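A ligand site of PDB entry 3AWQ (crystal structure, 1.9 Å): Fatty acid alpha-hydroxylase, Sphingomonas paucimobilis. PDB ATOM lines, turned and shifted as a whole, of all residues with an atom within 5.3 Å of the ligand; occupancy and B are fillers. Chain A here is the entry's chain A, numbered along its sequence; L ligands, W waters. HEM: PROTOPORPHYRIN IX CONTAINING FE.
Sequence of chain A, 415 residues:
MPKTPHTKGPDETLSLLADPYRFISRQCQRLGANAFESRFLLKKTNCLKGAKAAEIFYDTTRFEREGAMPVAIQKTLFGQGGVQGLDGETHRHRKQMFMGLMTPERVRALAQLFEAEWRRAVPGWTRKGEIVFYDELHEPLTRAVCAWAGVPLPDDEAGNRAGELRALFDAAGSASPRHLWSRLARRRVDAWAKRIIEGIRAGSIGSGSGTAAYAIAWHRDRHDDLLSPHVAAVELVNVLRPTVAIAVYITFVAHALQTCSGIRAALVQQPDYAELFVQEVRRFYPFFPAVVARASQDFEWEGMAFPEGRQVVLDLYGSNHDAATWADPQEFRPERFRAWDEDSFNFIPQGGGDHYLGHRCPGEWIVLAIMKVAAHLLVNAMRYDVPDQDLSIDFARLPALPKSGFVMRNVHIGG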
ATOM      1  N   PHE A  57      23.438  16.067   8.667  1.00  0.00           N
ATOM      2  CA  PHE A  57      22.356  15.897   7.689  1.00  0.00           C
ATOM      3  C   PHE A  57      22.911  15.421   6.352  1.00  0.00           C
ATOM      4  O   PHE A  57      22.283  14.618   5.659  1.00  0.00           O
ATOM      5  CB  PHE A  57      21.599  17.210   7.499  1.00  0.00           C
ATOM      6  CG  PHE A  57      20.371  17.096   6.618  1.00  0.00           C
ATOM      7  CD1 PHE A  57      19.156  16.680   7.163  1.00  0.00           C
ATOM      8  CD2 PHE A  57      20.431  17.429   5.247  1.00  0.00           C
ATOM      9  CE1 PHE A  57      17.989  16.607   6.345  1.00  0.00           C
ATOM     10  CE2 PHE A  57      19.284  17.358   4.431  1.00  0.00           C
ATOM     11  CZ  PHE A  57      18.061  16.932   4.966  1.00  0.00           C
ATOM     12  N   TYR A  58      24.111  15.914   6.014  1.00  0.00           N
ATOM     13  CA  TYR A  58      24.806  15.541   4.784  1.00  0.00           C
ATOM     14  C   TYR A  58      25.646  14.275   4.858  1.00  0.00           C
ATOM     15  O   TYR A  58      26.291  13.917   3.885  1.00  0.00           O
ATOM     16  CB  TYR A  58      25.590  16.736   4.222  1.00  0.00           C
ATOM     17  CG  TYR A  58      24.625  17.686   3.536  1.00  0.00           C
ATOM     18  CD1 TYR A  58      24.079  17.375   2.281  1.00  0.00           C
ATOM     19  CD2 TYR A  58      24.175  18.835   4.197  1.00  0.00           C
ATOM     20  CE1 TYR A  58      23.152  18.242   1.652  1.00  0.00           C
ATOM     21  CE2 TYR A  58      23.258  19.684   3.609  1.00  0.00           C
ATOM     22  CZ  TYR A  58      22.741  19.387   2.336  1.00  0.00           C
ATOM     23  OH  TYR A  58      21.850  20.261   1.769  1.00  0.00           O
ATOM     24  N   ARG A  65      17.413  10.062   0.898  1.00  0.00           N
ATOM     25  CA  ARG A  65      16.351  10.904   0.369  1.00  0.00           C
ATOM     26  C   ARG A  65      15.175  10.122  -0.215  1.00  0.00           C
ATOM     27  O   ARG A  65      14.084  10.676  -0.335  1.00  0.00           O
ATOM     28  CB  ARG A  65      16.895  11.841  -0.724  1.00  0.00           C
ATOM     29  CG  ARG A  65      18.094  12.722  -0.242  1.00  0.00           C
ATOM     30  CD  ARG A  65      17.780  13.522   1.043  1.00  0.00           C
ATOM     31  NE  ARG A  65      18.910  14.398   1.380  1.00  0.00           N
ATOM     32  CZ  ARG A  65      19.112  15.605   0.854  1.00  0.00           C
ATOM     33  NH1 ARG A  65      18.261  16.128  -0.020  1.00  0.00           N
ATOM     34  NH2 ARG A  65      20.181  16.323   1.221  1.00  0.00           N
ATOM     35  N   VAL A  83      16.805  13.358  -9.801  1.00  0.00           N
ATOM     36  CA  VAL A  83      17.992  13.132  -8.962  1.00  0.00           C
ATOM     37  C   VAL A  83      17.716  13.411  -7.467  1.00  0.00           C
ATOM     38  O   VAL A  83      18.355  12.818  -6.597  1.00  0.00           O
ATOM     39  CB  VAL A  83      19.160  14.026  -9.496  1.00  0.00           C
ATOM     40  CG1 VAL A  83      18.819  15.540  -9.380  1.00  0.00           C
ATOM     41  CG2 VAL A  83      20.511  13.724  -8.823  1.00  0.00           C
ATOM     42  N   GLN A  84      16.778  14.326  -7.166  1.00  0.00           N
ATOM     43  CA  GLN A  84      16.495  14.692  -5.734  1.00  0.00           C
ATOM     44  C   GLN A  84      16.086  13.500  -4.903  1.00  0.00           C
ATOM     45  O   GLN A  84      16.305  13.492  -3.682  1.00  0.00           O
ATOM     46  CB  GLN A  84      15.355  15.703  -5.632  1.00  0.00           C
ATOM     47  CG  GLN A  84      15.695  17.047  -6.232  1.00  0.00           C
ATOM     48  CD  GLN A  84      15.214  17.161  -7.676  1.00  0.00           C
ATOM     49  OE1 GLN A  84      14.917  16.143  -8.338  1.00  0.00           O
ATOM     50  NE2 GLN A  84      15.117  18.390  -8.165  1.00  0.00           N
ATOM     51  N   HIS A  91      22.503   7.735  -7.133  1.00  0.00           N
ATOM     52  CA  HIS A  91      22.485   9.201  -7.042  1.00  0.00           C
ATOM     53  C   HIS A  91      23.754   9.815  -7.599  1.00  0.00           C
ATOM     54  O   HIS A  91      23.703  10.785  -8.367  1.00  0.00           O
ATOM     55  CB  HIS A  91      22.284   9.700  -5.608  1.00  0.00           C
ATOM     56  CG  HIS A  91      22.534  11.174  -5.467  1.00  0.00           C
ATOM     57  ND1 HIS A  91      23.712  11.690  -4.975  1.00  0.00           N
ATOM     58  CD2 HIS A  91      21.787  12.227  -5.859  1.00  0.00           C
ATOM     59  CE1 HIS A  91      23.663  13.014  -5.032  1.00  0.00           C
ATOM     60  NE2 HIS A  91      22.497  13.368  -5.552  1.00  0.00           N
ATOM     61  N   LYS A  95      24.049  12.489 -10.484  1.00  0.00           N
ATOM     62  CA  LYS A  95      24.531  13.844 -10.101  1.00  0.00           C
ATOM     63  C   LYS A  95      25.683  14.325 -11.024  1.00  0.00           C
ATOM     64  O   LYS A  95      25.739  15.498 -11.409  1.00  0.00           O
ATOM     65  CB  LYS A  95      24.931  13.861  -8.627  1.00  0.00           C
ATOM     66  CG  LYS A  95      25.369  15.247  -8.097  1.00  0.00           C
ATOM     67  CD  LYS A  95      24.252  16.284  -8.375  1.00  0.00           C
ATOM     68  CE  LYS A  95      24.500  17.594  -7.597  1.00  0.00           C
ATOM     69  NZ  LYS A  95      24.252  17.401  -6.134  1.00  0.00           N
ATOM     70  N   PHE A  98      24.629  16.233 -14.075  1.00  0.00           N
ATOM     71  CA  PHE A  98      24.387  17.662 -13.899  1.00  0.00           C
ATOM     72  C   PHE A  98      25.692  18.444 -13.716  1.00  0.00           C
ATOM     73  O   PHE A  98      25.839  19.552 -14.263  1.00  0.00           O
ATOM     74  CB  PHE A  98      23.495  17.926 -12.680  1.00  0.00           C
ATOM     75  CG  PHE A  98      22.047  17.537 -12.896  1.00  0.00           C
ATOM     76  CD1 PHE A  98      21.166  18.430 -13.513  1.00  0.00           C
ATOM     77  CD2 PHE A  98      21.584  16.289 -12.478  1.00  0.00           C
ATOM     78  CE1 PHE A  98      19.810  18.086 -13.704  1.00  0.00           C
ATOM     79  CE2 PHE A  98      20.211  15.922 -12.660  1.00  0.00           C
ATOM     80  CZ  PHE A  98      19.329  16.826 -13.277  1.00  0.00           C
ATOM     81  N   MET A 102      28.409  22.230 -15.814  1.00  0.00           N
ATOM     82  CA  MET A 102      28.742  23.487 -15.128  1.00  0.00           C
ATOM     83  C   MET A 102      30.185  23.969 -15.306  1.00  0.00           C
ATOM     84  O   MET A 102      30.789  24.536 -14.377  1.00  0.00           O
ATOM     85  CB  MET A 102      28.444  23.339 -13.620  1.00  0.00           C
ATOM     86  CG  MET A 102      27.004  22.790 -13.359  1.00  0.00           C
ATOM     87  SD  MET A 102      25.808  23.779 -14.283  1.00  0.00           S
ATOM     88  CE  MET A 102      24.320  22.932 -13.755  1.00  0.00           C
ATOM     89  N   ASN A 238      14.576  19.826 -14.393  1.00  0.00           N
ATOM     90  CA  ASN A 238      15.450  20.166 -13.255  1.00  0.00           C
ATOM     91  C   ASN A 238      16.584  21.135 -13.604  1.00  0.00           C
ATOM     92  O   ASN A 238      17.277  21.591 -12.704  1.00  0.00           O
ATOM     93  CB  ASN A 238      16.048  18.882 -12.597  1.00  0.00           C
ATOM     94  CG  ASN A 238      15.095  18.249 -11.604  1.00  0.00           C
ATOM     95  OD1 ASN A 238      14.275  18.952 -10.976  1.00  0.00           O
ATOM     96  ND2 ASN A 238      15.197  16.927 -11.433  1.00  0.00           N
ATOM     97  N   VAL A 239      16.819  21.404 -14.889  1.00  0.00           N
ATOM     98  CA  VAL A 239      17.719  22.490 -15.299  1.00  0.00           C
ATOM     99  C   VAL A 239      16.914  23.770 -15.612  1.00  0.00           C
ATOM    100  O   VAL A 239      17.254  24.868 -15.130  1.00  0.00           O
ATOM    101  CB  VAL A 239      18.579  22.099 -16.536  1.00  0.00           C
ATOM    102  CG1 VAL A 239      19.495  23.306 -16.988  1.00  0.00           C
ATOM    103  CG2 VAL A 239      19.468  20.861 -16.218  1.00  0.00           C
ATOM    104  N   PRO A 242      14.703  25.593 -12.245  1.00  0.00           N
ATOM    105  CA  PRO A 242      15.345  26.412 -11.210  1.00  0.00           C
ATOM    106  C   PRO A 242      16.105  27.581 -11.814  1.00  0.00           C
ATOM    107  O   PRO A 242      16.314  28.568 -11.128  1.00  0.00           O
ATOM    108  CB  PRO A 242      16.324  25.443 -10.533  1.00  0.00           C
ATOM    109  CG  PRO A 242      16.121  24.157 -11.139  1.00  0.00           C
ATOM    110  CD  PRO A 242      15.222  24.217 -12.291  1.00  0.00           C
ATOM    111  N   THR A 243      16.510  27.501 -13.085  1.00  0.00           N
ATOM    112  CA  THR A 243      17.117  28.697 -13.731  1.00  0.00           C
ATOM    113  C   THR A 243      16.112  29.850 -13.814  1.00  0.00           C
ATOM    114  O   THR A 243      16.443  31.029 -13.527  1.00  0.00           O
ATOM    115  CB  THR A 243      17.726  28.367 -15.119  1.00  0.00           C
ATOM    116  OG1 THR A 243      18.656  27.288 -14.974  1.00  0.00           O
ATOM    117  CG2 THR A 243      18.502  29.559 -15.712  1.00  0.00           C
ATOM    118  N   ALA A 245      13.682  30.183 -11.729  1.00  0.00           N
ATOM    119  CA  ALA A 245      13.505  30.593 -10.321  1.00  0.00           C
ATOM    120  C   ALA A 245      14.521  31.641  -9.858  1.00  0.00           C
ATOM    121  O   ALA A 245      14.349  32.260  -8.787  1.00  0.00           O
ATOM    122  CB  ALA A 245      13.539  29.366  -9.375  1.00  0.00           C
ATOM    123  N   ILE A 246      15.593  31.815 -10.626  1.00  0.00           N
ATOM    124  CA  ILE A 246      16.572  32.912 -10.318  1.00  0.00           C
ATOM    125  C   ILE A 246      15.876  34.281 -10.334  1.00  0.00           C
ATOM    126  O   ILE A 246      16.356  35.232  -9.697  1.00  0.00           O
ATOM    127  CB  ILE A 246      17.826  32.862 -11.215  1.00  0.00           C
ATOM    128  CG1 ILE A 246      18.533  31.490 -11.067  1.00  0.00           C
ATOM    129  CG2 ILE A 246      18.836  33.978 -10.805  1.00  0.00           C
ATOM    130  CD1 ILE A 246      19.606  31.228 -12.122  1.00  0.00           C
ATOM    131  N   TYR A 249      15.850  35.590  -6.807  1.00  0.00           N
ATOM    132  CA  TYR A 249      17.095  36.234  -6.354  1.00  0.00           C
ATOM    133  C   TYR A 249      17.331  37.570  -7.042  1.00  0.00           C
ATOM    134  O   TYR A 249      17.836  38.495  -6.413  1.00  0.00           O
ATOM    135  CB  TYR A 249      18.298  35.348  -6.596  1.00  0.00           C
ATOM    136  CG  TYR A 249      18.595  34.396  -5.469  1.00  0.00           C
ATOM    137  CD1 TYR A 249      18.483  34.803  -4.116  1.00  0.00           C
ATOM    138  CD2 TYR A 249      19.029  33.090  -5.745  1.00  0.00           C
ATOM    139  CE1 TYR A 249      18.786  33.919  -3.071  1.00  0.00           C
ATOM    140  CE2 TYR A 249      19.354  32.199  -4.708  1.00  0.00           C
ATOM    141  CZ  TYR A 249      19.232  32.623  -3.387  1.00  0.00           C
ATOM    142  OH  TYR A 249      19.531  31.769  -2.353  1.00  0.00           O
ATOM    143  N   PHE A 287      14.618  31.945   0.674  1.00  0.00           N
ATOM    144  CA  PHE A 287      14.224  31.441  -0.643  1.00  0.00           C
ATOM    145  C   PHE A 287      13.854  29.962  -0.502  1.00  0.00           C
ATOM    146  O   PHE A 287      12.668  29.599  -0.478  1.00  0.00           O
ATOM    147  CB  PHE A 287      15.364  31.694  -1.659  1.00  0.00           C
ATOM    148  CG  PHE A 287      14.972  31.467  -3.126  1.00  0.00           C
ATOM    149  CD1 PHE A 287      13.820  30.759  -3.470  1.00  0.00           C
ATOM    150  CD2 PHE A 287      15.799  31.930  -4.143  1.00  0.00           C
ATOM    151  CE1 PHE A 287      13.478  30.553  -4.823  1.00  0.00           C
ATOM    152  CE2 PHE A 287      15.489  31.709  -5.483  1.00  0.00           C
ATOM    153  CZ  PHE A 287      14.336  31.011  -5.838  1.00  0.00           C
ATOM    154  N   PHE A 288      14.857  29.094  -0.378  1.00  0.00           N
ATOM    155  CA  PHE A 288      14.570  27.667  -0.233  1.00  0.00           C
ATOM    156  C   PHE A 288      14.480  27.416   1.264  1.00  0.00           C
ATOM    157  O   PHE A 288      15.446  27.599   1.982  1.00  0.00           O
ATOM    158  CB  PHE A 288      15.673  26.831  -0.865  1.00  0.00           C
ATOM    159  CG  PHE A 288      15.205  25.475  -1.307  1.00  0.00           C
ATOM    160  CD1 PHE A 288      14.912  24.485  -0.364  1.00  0.00           C
ATOM    161  CD2 PHE A 288      15.088  25.179  -2.661  1.00  0.00           C
ATOM    162  CE1 PHE A 288      14.460  23.214  -0.767  1.00  0.00           C
ATOM    163  CE2 PHE A 288      14.660  23.899  -3.092  1.00  0.00           C
ATOM    164  CZ  PHE A 288      14.354  22.919  -2.130  1.00  0.00           C
ATOM    165  N   VAL A 291      15.249  21.455   3.734  1.00  0.00           N
ATOM    166  CA  VAL A 291      15.394  20.229   2.952  1.00  0.00           C
ATOM    167  C   VAL A 291      15.028  19.056   3.866  1.00  0.00           C
ATOM    168  O   VAL A 291      15.215  19.144   5.071  1.00  0.00           O
ATOM    169  CB  VAL A 291      16.836  20.100   2.422  1.00  0.00           C
ATOM    170  CG1 VAL A 291      17.105  18.715   1.785  1.00  0.00           C
ATOM    171  CG2 VAL A 291      17.110  21.204   1.383  1.00  0.00           C
ATOM    172  N   LEU A 316      17.399  25.684   6.225  1.00  0.00           N
ATOM    173  CA  LEU A 316      18.436  26.451   5.505  1.00  0.00           C
ATOM    174  C   LEU A 316      18.464  27.927   5.910  1.00  0.00           C
ATOM    175  O   LEU A 316      19.520  28.487   6.192  1.00  0.00           O
ATOM    176  CB  LEU A 316      18.203  26.344   3.986  1.00  0.00           C
ATOM    177  CG  LEU A 316      18.219  24.918   3.422  1.00  0.00           C
ATOM    178  CD1 LEU A 316      18.104  25.007   1.865  1.00  0.00           C
ATOM    179  CD2 LEU A 316      19.456  24.096   3.872  1.00  0.00           C
ATOM    180  N   PRO A 349      22.423  28.314   1.388  1.00  0.00           N
ATOM    181  CA  PRO A 349      21.151  28.749   0.757  1.00  0.00           C
ATOM    182  C   PRO A 349      20.686  27.789  -0.370  1.00  0.00           C
ATOM    183  O   PRO A 349      19.491  27.743  -0.699  1.00  0.00           O
ATOM    184  CB  PRO A 349      21.511  30.106   0.147  1.00  0.00           C
ATOM    185  CG  PRO A 349      23.005  29.984  -0.138  1.00  0.00           C
ATOM    186  CD  PRO A 349      23.532  29.229   1.060  1.00  0.00           C
ATOM    187  N   GLN A 350      21.632  27.025  -0.927  1.00  0.00           N
ATOM    188  CA  GLN A 350      21.338  26.022  -1.949  1.00  0.00           C
ATOM    189  C   GLN A 350      21.889  24.682  -1.513  1.00  0.00           C
ATOM    190  O   GLN A 350      22.342  23.870  -2.315  1.00  0.00           O
ATOM    191  CB  GLN A 350      21.883  26.502  -3.319  1.00  0.00           C
ATOM    192  CG  GLN A 350      21.213  27.878  -3.725  1.00  0.00           C
ATOM    193  CD  GLN A 350      21.657  28.427  -5.074  1.00  0.00           C
ATOM    194  OE1 GLN A 350      22.049  29.587  -5.173  1.00  0.00           O
ATOM    195  NE2 GLN A 350      21.615  27.588  -6.124  1.00  0.00           N
ATOM    196  N   GLY A 351      21.822  24.426  -0.205  1.00  0.00           N
ATOM    197  CA  GLY A 351      22.325  23.164   0.335  1.00  0.00           C
ATOM    198  C   GLY A 351      23.773  23.210   0.803  1.00  0.00           C
ATOM    199  O   GLY A 351      24.497  24.176   0.545  1.00  0.00           O
ATOM    200  N   GLY A 352      24.199  22.145   1.462  1.00  0.00           N
ATOM    201  CA  GLY A 352      25.536  22.050   2.067  1.00  0.00           C
ATOM    202  C   GLY A 352      26.240  20.802   1.589  1.00  0.00           C
ATOM    203  O   GLY A 352      25.707  20.028   0.781  1.00  0.00           O
ATOM    204  N   GLY A 358      26.931  14.465  -2.567  1.00  0.00           N
ATOM    205  CA  GLY A 358      25.659  14.684  -1.897  1.00  0.00           C
ATOM    206  C   GLY A 358      24.700  15.475  -2.777  1.00  0.00           C
ATOM    207  O   GLY A 358      24.966  15.683  -3.948  1.00  0.00           O
ATOM    208  N   HIS A 359      23.593  15.925  -2.182  1.00  0.00           N
ATOM    209  CA  HIS A 359      22.487  16.540  -2.937  1.00  0.00           C
ATOM    210  C   HIS A 359      22.599  18.073  -3.110  1.00  0.00           C
ATOM    211  O   HIS A 359      21.675  18.713  -3.611  1.00  0.00           O
ATOM    212  CB  HIS A 359      21.147  16.173  -2.283  1.00  0.00           C
ATOM    213  CG  HIS A 359      20.756  14.745  -2.537  1.00  0.00           C
ATOM    214  ND1 HIS A 359      19.962  14.369  -3.597  1.00  0.00           N
ATOM    215  CD2 HIS A 359      21.103  13.607  -1.892  1.00  0.00           C
ATOM    216  CE1 HIS A 359      19.811  13.055  -3.586  1.00  0.00           C
ATOM    217  NE2 HIS A 359      20.505  12.568  -2.565  1.00  0.00           N
ATOM    218  N   ARG A 360      23.726  18.639  -2.693  1.00  0.00           N
ATOM    219  CA  ARG A 360      23.938  20.086  -2.824  1.00  0.00           C
ATOM    220  C   ARG A 360      23.650  20.551  -4.256  1.00  0.00           C
ATOM    221  O   ARG A 360      24.009  19.861  -5.250  1.00  0.00           O
ATOM    222  CB  ARG A 360      25.401  20.443  -2.466  1.00  0.00           C
ATOM    223  CG  ARG A 360      25.651  21.974  -2.437  1.00  0.00           C
ATOM    224  CD  ARG A 360      27.106  22.254  -1.946  1.00  0.00           C
ATOM    225  NE  ARG A 360      27.281  23.716  -1.870  1.00  0.00           N
ATOM    226  CZ  ARG A 360      27.786  24.355  -0.820  1.00  0.00           C
ATOM    227  NH1 ARG A 360      28.250  23.686   0.240  1.00  0.00           N
ATOM    228  NH2 ARG A 360      27.858  25.676  -0.858  1.00  0.00           N
ATOM    229  N   CYS A 361      23.009  21.712  -4.352  1.00  0.00           N
ATOM    230  CA  CYS A 361      22.595  22.287  -5.656  1.00  0.00           C
ATOM    231  C   CYS A 361      23.758  22.442  -6.668  1.00  0.00           C
ATOM    232  O   CYS A 361      24.734  23.153  -6.407  1.00  0.00           O
ATOM    233  CB  CYS A 361      21.943  23.652  -5.428  1.00  0.00           C
ATOM    234  SG  CYS A 361      21.394  24.441  -6.960  1.00  0.00           S
ATOM    235  N   PRO A 362      23.657  21.802  -7.848  1.00  0.00           N
ATOM    236  CA  PRO A 362      24.706  21.973  -8.849  1.00  0.00           C
ATOM    237  C   PRO A 362      24.529  23.321  -9.588  1.00  0.00           C
ATOM    238  O   PRO A 362      25.394  23.688 -10.378  1.00  0.00           O
ATOM    239  CB  PRO A 362      24.450  20.815  -9.823  1.00  0.00           C
ATOM    240  CG  PRO A 362      22.899  20.666  -9.784  1.00  0.00           C
ATOM    241  CD  PRO A 362      22.547  20.923  -8.314  1.00  0.00           C
ATOM    242  N   GLY A 363      23.421  24.020  -9.323  1.00  0.00           N
ATOM    243  CA  GLY A 363      23.122  25.273  -9.999  1.00  0.00           C
ATOM    244  C   GLY A 363      23.789  26.501  -9.407  1.00  0.00           C
ATOM    245  O   GLY A 363      23.578  27.613  -9.900  1.00  0.00           O
ATOM    246  N   ILE A 366      25.746  28.927 -11.818  1.00  0.00           N
ATOM    247  CA  ILE A 366      24.795  29.640 -12.675  1.00  0.00           C
ATOM    248  C   ILE A 366      24.108  30.762 -11.890  1.00  0.00           C
ATOM    249  O   ILE A 366      24.011  31.910 -12.356  1.00  0.00           O
ATOM    250  CB  ILE A 366      23.728  28.670 -13.275  1.00  0.00           C
ATOM    251  CG1 ILE A 366      24.381  27.785 -14.331  1.00  0.00           C
ATOM    252  CG2 ILE A 366      22.513  29.460 -13.833  1.00  0.00           C
ATOM    253  CD1 ILE A 366      23.517  26.568 -14.737  1.00  0.00           C
ATOM    254  N   VAL A 367      23.587  30.418 -10.714  1.00  0.00           N
ATOM    255  CA  VAL A 367      22.934  31.415  -9.882  1.00  0.00           C
ATOM    256  C   VAL A 367      23.862  32.613  -9.621  1.00  0.00           C
ATOM    257  O   VAL A 367      23.449  33.781  -9.811  1.00  0.00           O
ATOM    258  CB  VAL A 367      22.416  30.835  -8.558  1.00  0.00           C
ATOM    259  CG1 VAL A 367      21.957  31.975  -7.606  1.00  0.00           C
ATOM    260  CG2 VAL A 367      21.233  29.884  -8.846  1.00  0.00           C
HETATM  261  CHA HEM L   1      19.131  21.045  -5.453  1.00  0.00           C
HETATM  262  CHB HEM L   1      18.338  25.601  -4.087  1.00  0.00           C
HETATM  263  CHC HEM L   1      19.046  27.108  -8.648  1.00  0.00           C
HETATM  264  CHD HEM L   1      19.537  22.516 -10.117  1.00  0.00           C
HETATM  265  C1A HEM L   1      18.900  22.158  -4.674  1.00  0.00           C
HETATM  266  C2A HEM L   1      18.709  22.153  -3.244  1.00  0.00           C
HETATM  267  C3A HEM L   1      18.504  23.425  -2.849  1.00  0.00           C
HETATM  268  C4A HEM L   1      18.544  24.247  -4.047  1.00  0.00           C
HETATM  269  CMA HEM L   1      18.221  23.942  -1.432  1.00  0.00           C
HETATM  270  CAA HEM L   1      18.677  20.872  -2.391  1.00  0.00           C
HETATM  271  CBA HEM L   1      19.934  20.584  -1.565  1.00  0.00           C
HETATM  272  CGA HEM L   1      19.659  19.242  -0.890  1.00  0.00           C
HETATM  273  O1A HEM L   1      20.439  18.913   0.032  1.00  0.00           O
HETATM  274  O2A HEM L   1      18.697  18.488  -1.268  1.00  0.00           O
HETATM  275  C1B HEM L   1      18.337  26.392  -5.206  1.00  0.00           C
HETATM  276  C2B HEM L   1      17.972  27.795  -5.249  1.00  0.00           C
HETATM  277  C3B HEM L   1      18.147  28.198  -6.524  1.00  0.00           C
HETATM  278  C4B HEM L   1      18.642  27.080  -7.313  1.00  0.00           C
HETATM  279  CMB HEM L   1      17.463  28.666  -4.052  1.00  0.00           C
HETATM  280  CAB HEM L   1      17.893  29.626  -7.041  1.00  0.00           C
HETATM  281  CBB HEM L   1      17.145  29.863  -8.098  1.00  0.00           C
HETATM  282  C1C HEM L   1      19.374  26.028  -9.441  1.00  0.00           C
HETATM  283  C2C HEM L   1      19.772  26.053 -10.837  1.00  0.00           C
HETATM  284  C3C HEM L   1      19.918  24.782 -11.256  1.00  0.00           C
HETATM  285  C4C HEM L   1      19.597  23.907 -10.138  1.00  0.00           C
HETATM  286  CMC HEM L   1      20.022  27.312 -11.702  1.00  0.00           C
HETATM  287  CAC HEM L   1      20.327  24.392 -12.697  1.00  0.00           C
HETATM  288  CBC HEM L   1      21.007  23.272 -12.941  1.00  0.00           C
HETATM  289  C1D HEM L   1      19.369  21.712  -9.009  1.00  0.00           C
HETATM  290  C2D HEM L   1      19.301  20.257  -9.047  1.00  0.00           C
HETATM  291  C3D HEM L   1      19.170  19.816  -7.607  1.00  0.00           C
HETATM  292  C4D HEM L   1      19.190  21.024  -6.823  1.00  0.00           C
HETATM  293  CMD HEM L   1      19.313  19.346 -10.290  1.00  0.00           C
HETATM  294  CAD HEM L   1      19.082  18.381  -7.096  1.00  0.00           C
HETATM  295  CBD HEM L   1      20.579  17.979  -6.870  1.00  0.00           C
HETATM  296  CGD HEM L   1      20.664  16.638  -6.137  1.00  0.00           C
HETATM  297  O1D HEM L   1      21.761  16.012  -6.095  1.00  0.00           O
HETATM  298  O2D HEM L   1      19.626  16.177  -5.568  1.00  0.00           O
HETATM  299  NA  HEM L   1      18.794  23.447  -5.136  1.00  0.00           N
HETATM  300  NB  HEM L   1      18.746  25.989  -6.477  1.00  0.00           N
HETATM  301  NC  HEM L   1      19.309  24.702  -9.051  1.00  0.00           N
HETATM  302  ND  HEM L   1      19.329  22.127  -7.681  1.00  0.00           N
HETATM  303 FE   HEM L   1      19.115  24.084  -7.079  1.00  0.00          FE
HETATM  304  O   HOH W   1      15.829  21.116  -6.706  1.00  0.00           O
HETATM  305  O   HOH W   2      15.926  18.749  -1.675  1.00  0.00           O
HETATM  306  O   HOH W   3      17.826  17.575  -3.762  1.00  0.00           O
HETATM  307  O   HOH W   4      16.275  21.089  -9.692  1.00  0.00           O
HETATM  308  O   HOH W   5      16.009  19.821  -4.253  1.00  0.00           O
HETATM  309  O   HOH W   6      17.011  23.760  -7.467  1.00  0.00           O
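SG of Cys 361 binds FE of the ligand, at 2.3 Å.
An oxygen (O1A) of the ligand is in hydrogen-bond range of the side-chain hydroxyl (OH) of Tyr 58.
ND1 of His 359 is in hydrogen-bond range of O2D of the ligand.
NH1 of Arg 65 is in salt-bridge range of O2A of the ligand.
A ring nitrogen (NE2) of His 91 lies within hydrogen-bond range of an oxygen (O1D) of the ligand, at 2.8 Å.
The side-chain amino group (NZ) of Lys 95 lies within salt-bridge range of an oxygen (O1D) of the ligand (2.9 Å).
The backbone carbonyl oxygen (O) of Gln 350 lies within hydrogen-bond range of the backbone NH (N) of Cys 361 (3.0 Å).
The backbone NH of Gly 363 lies close to the side-chain sulfur of Cys 361 (3.1 Å).
N of Gly 352 is in hydrogen-bond range of OH of Tyr 58 (3.0 Å).
A ring nitrogen (NE2) of His 91 sits close to a ring nitrogen (ND1) of His 359, 3.4 Å away.
O of Gly 358 sits at hydrogen-bond distance from NZ of Lys 95.
The side-chain amino group (NZ) of Lys 95 sits at hydrogen-bond distance from the backbone carbonyl oxygen (O) of Arg 360.
The side-chain amide oxygen of Asn 238 lies within hydrogen-bond range of the side-chain amide nitrogen of Gln 84 (3.0 Å).
The backbone carbonyl oxygen (O) of Val 239 lies within hydrogen-bond range of the side-chain hydroxyl (OG1) of Thr 243, at 2.8 Å.
NB of the ligand sits close to NE2 of Gln 350.
Val 83 touches the ligand (CG1 to CAD, 3.7 Å).
Gln 84 touches the ligand.
CE1 of Phe 98 touches CMD of the ligand, at 3.7 Å.
Met 102 touches the ligand (CE to CBC, 3.4 Å).
O of Asn 238 touches CHD of the ligand, 3.6 Å away.
O of Val 239 touches CAC of the ligand, 3.9 Å away.
CB of Pro 242 touches C1C of the ligand, at 3.3 Å.
Thr 243 touches the ligand.
Ala 245 touches the ligand.
Ile 246 touches the ligand.
Tyr 249 touches the ligand (CE2 to CAB, 3.8 Å).
Phe 287 touches the ligand (CE2 to CAB, 3.5 Å).
Phe 288 touches the ligand.
Val 291 touches the ligand.
Leu 316 touches the ligand (CD1 to CMA, 3.5 Å).
Gly 351 touches the ligand.
Gly 358 touches the ligand.
Pro 362 touches the ligand (CD to C1D, 3.3 Å).
Gly 363 touches the ligand.
CG2 of Ile 366 touches CMC of the ligand (3.9 Å).
Val 367 touches the ligand.
Hydrophobic or aromatic side chains within 4 Å of the ligand: Tyr 58, Val 83, His 91, Phe 98, Met 102, Pro 242, Ala 245, Ile 246, Tyr 249, Phe 287, Phe 288, Val 291, Leu 316, His 359, Pro 362, Ile 366 and Val 367.
Within 4 Å of the ligand: Tyr 58, Arg 65, Val 83, Gln 84, His 91, Lys 95, Phe 98, Met 102, Asn 238, Val 239, Pro 242, Thr 243, Ala 245, Ile 246, Tyr 249, Phe 287, Phe 288, Val 291, Leu 316, Gln 350, Gly 351, Gly 358, His 359, Cys 361, Pro 362, Gly 363, Ile 366 and Val 367.
The nearest printed residue that does not touch the ligand is Pro 349 (4.03 Å).
Water W4 lies within hydrogen-bond range of OD1 of Asn 238 (3.2 Å) and NE2 of Gln 84 (3.3 Å).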
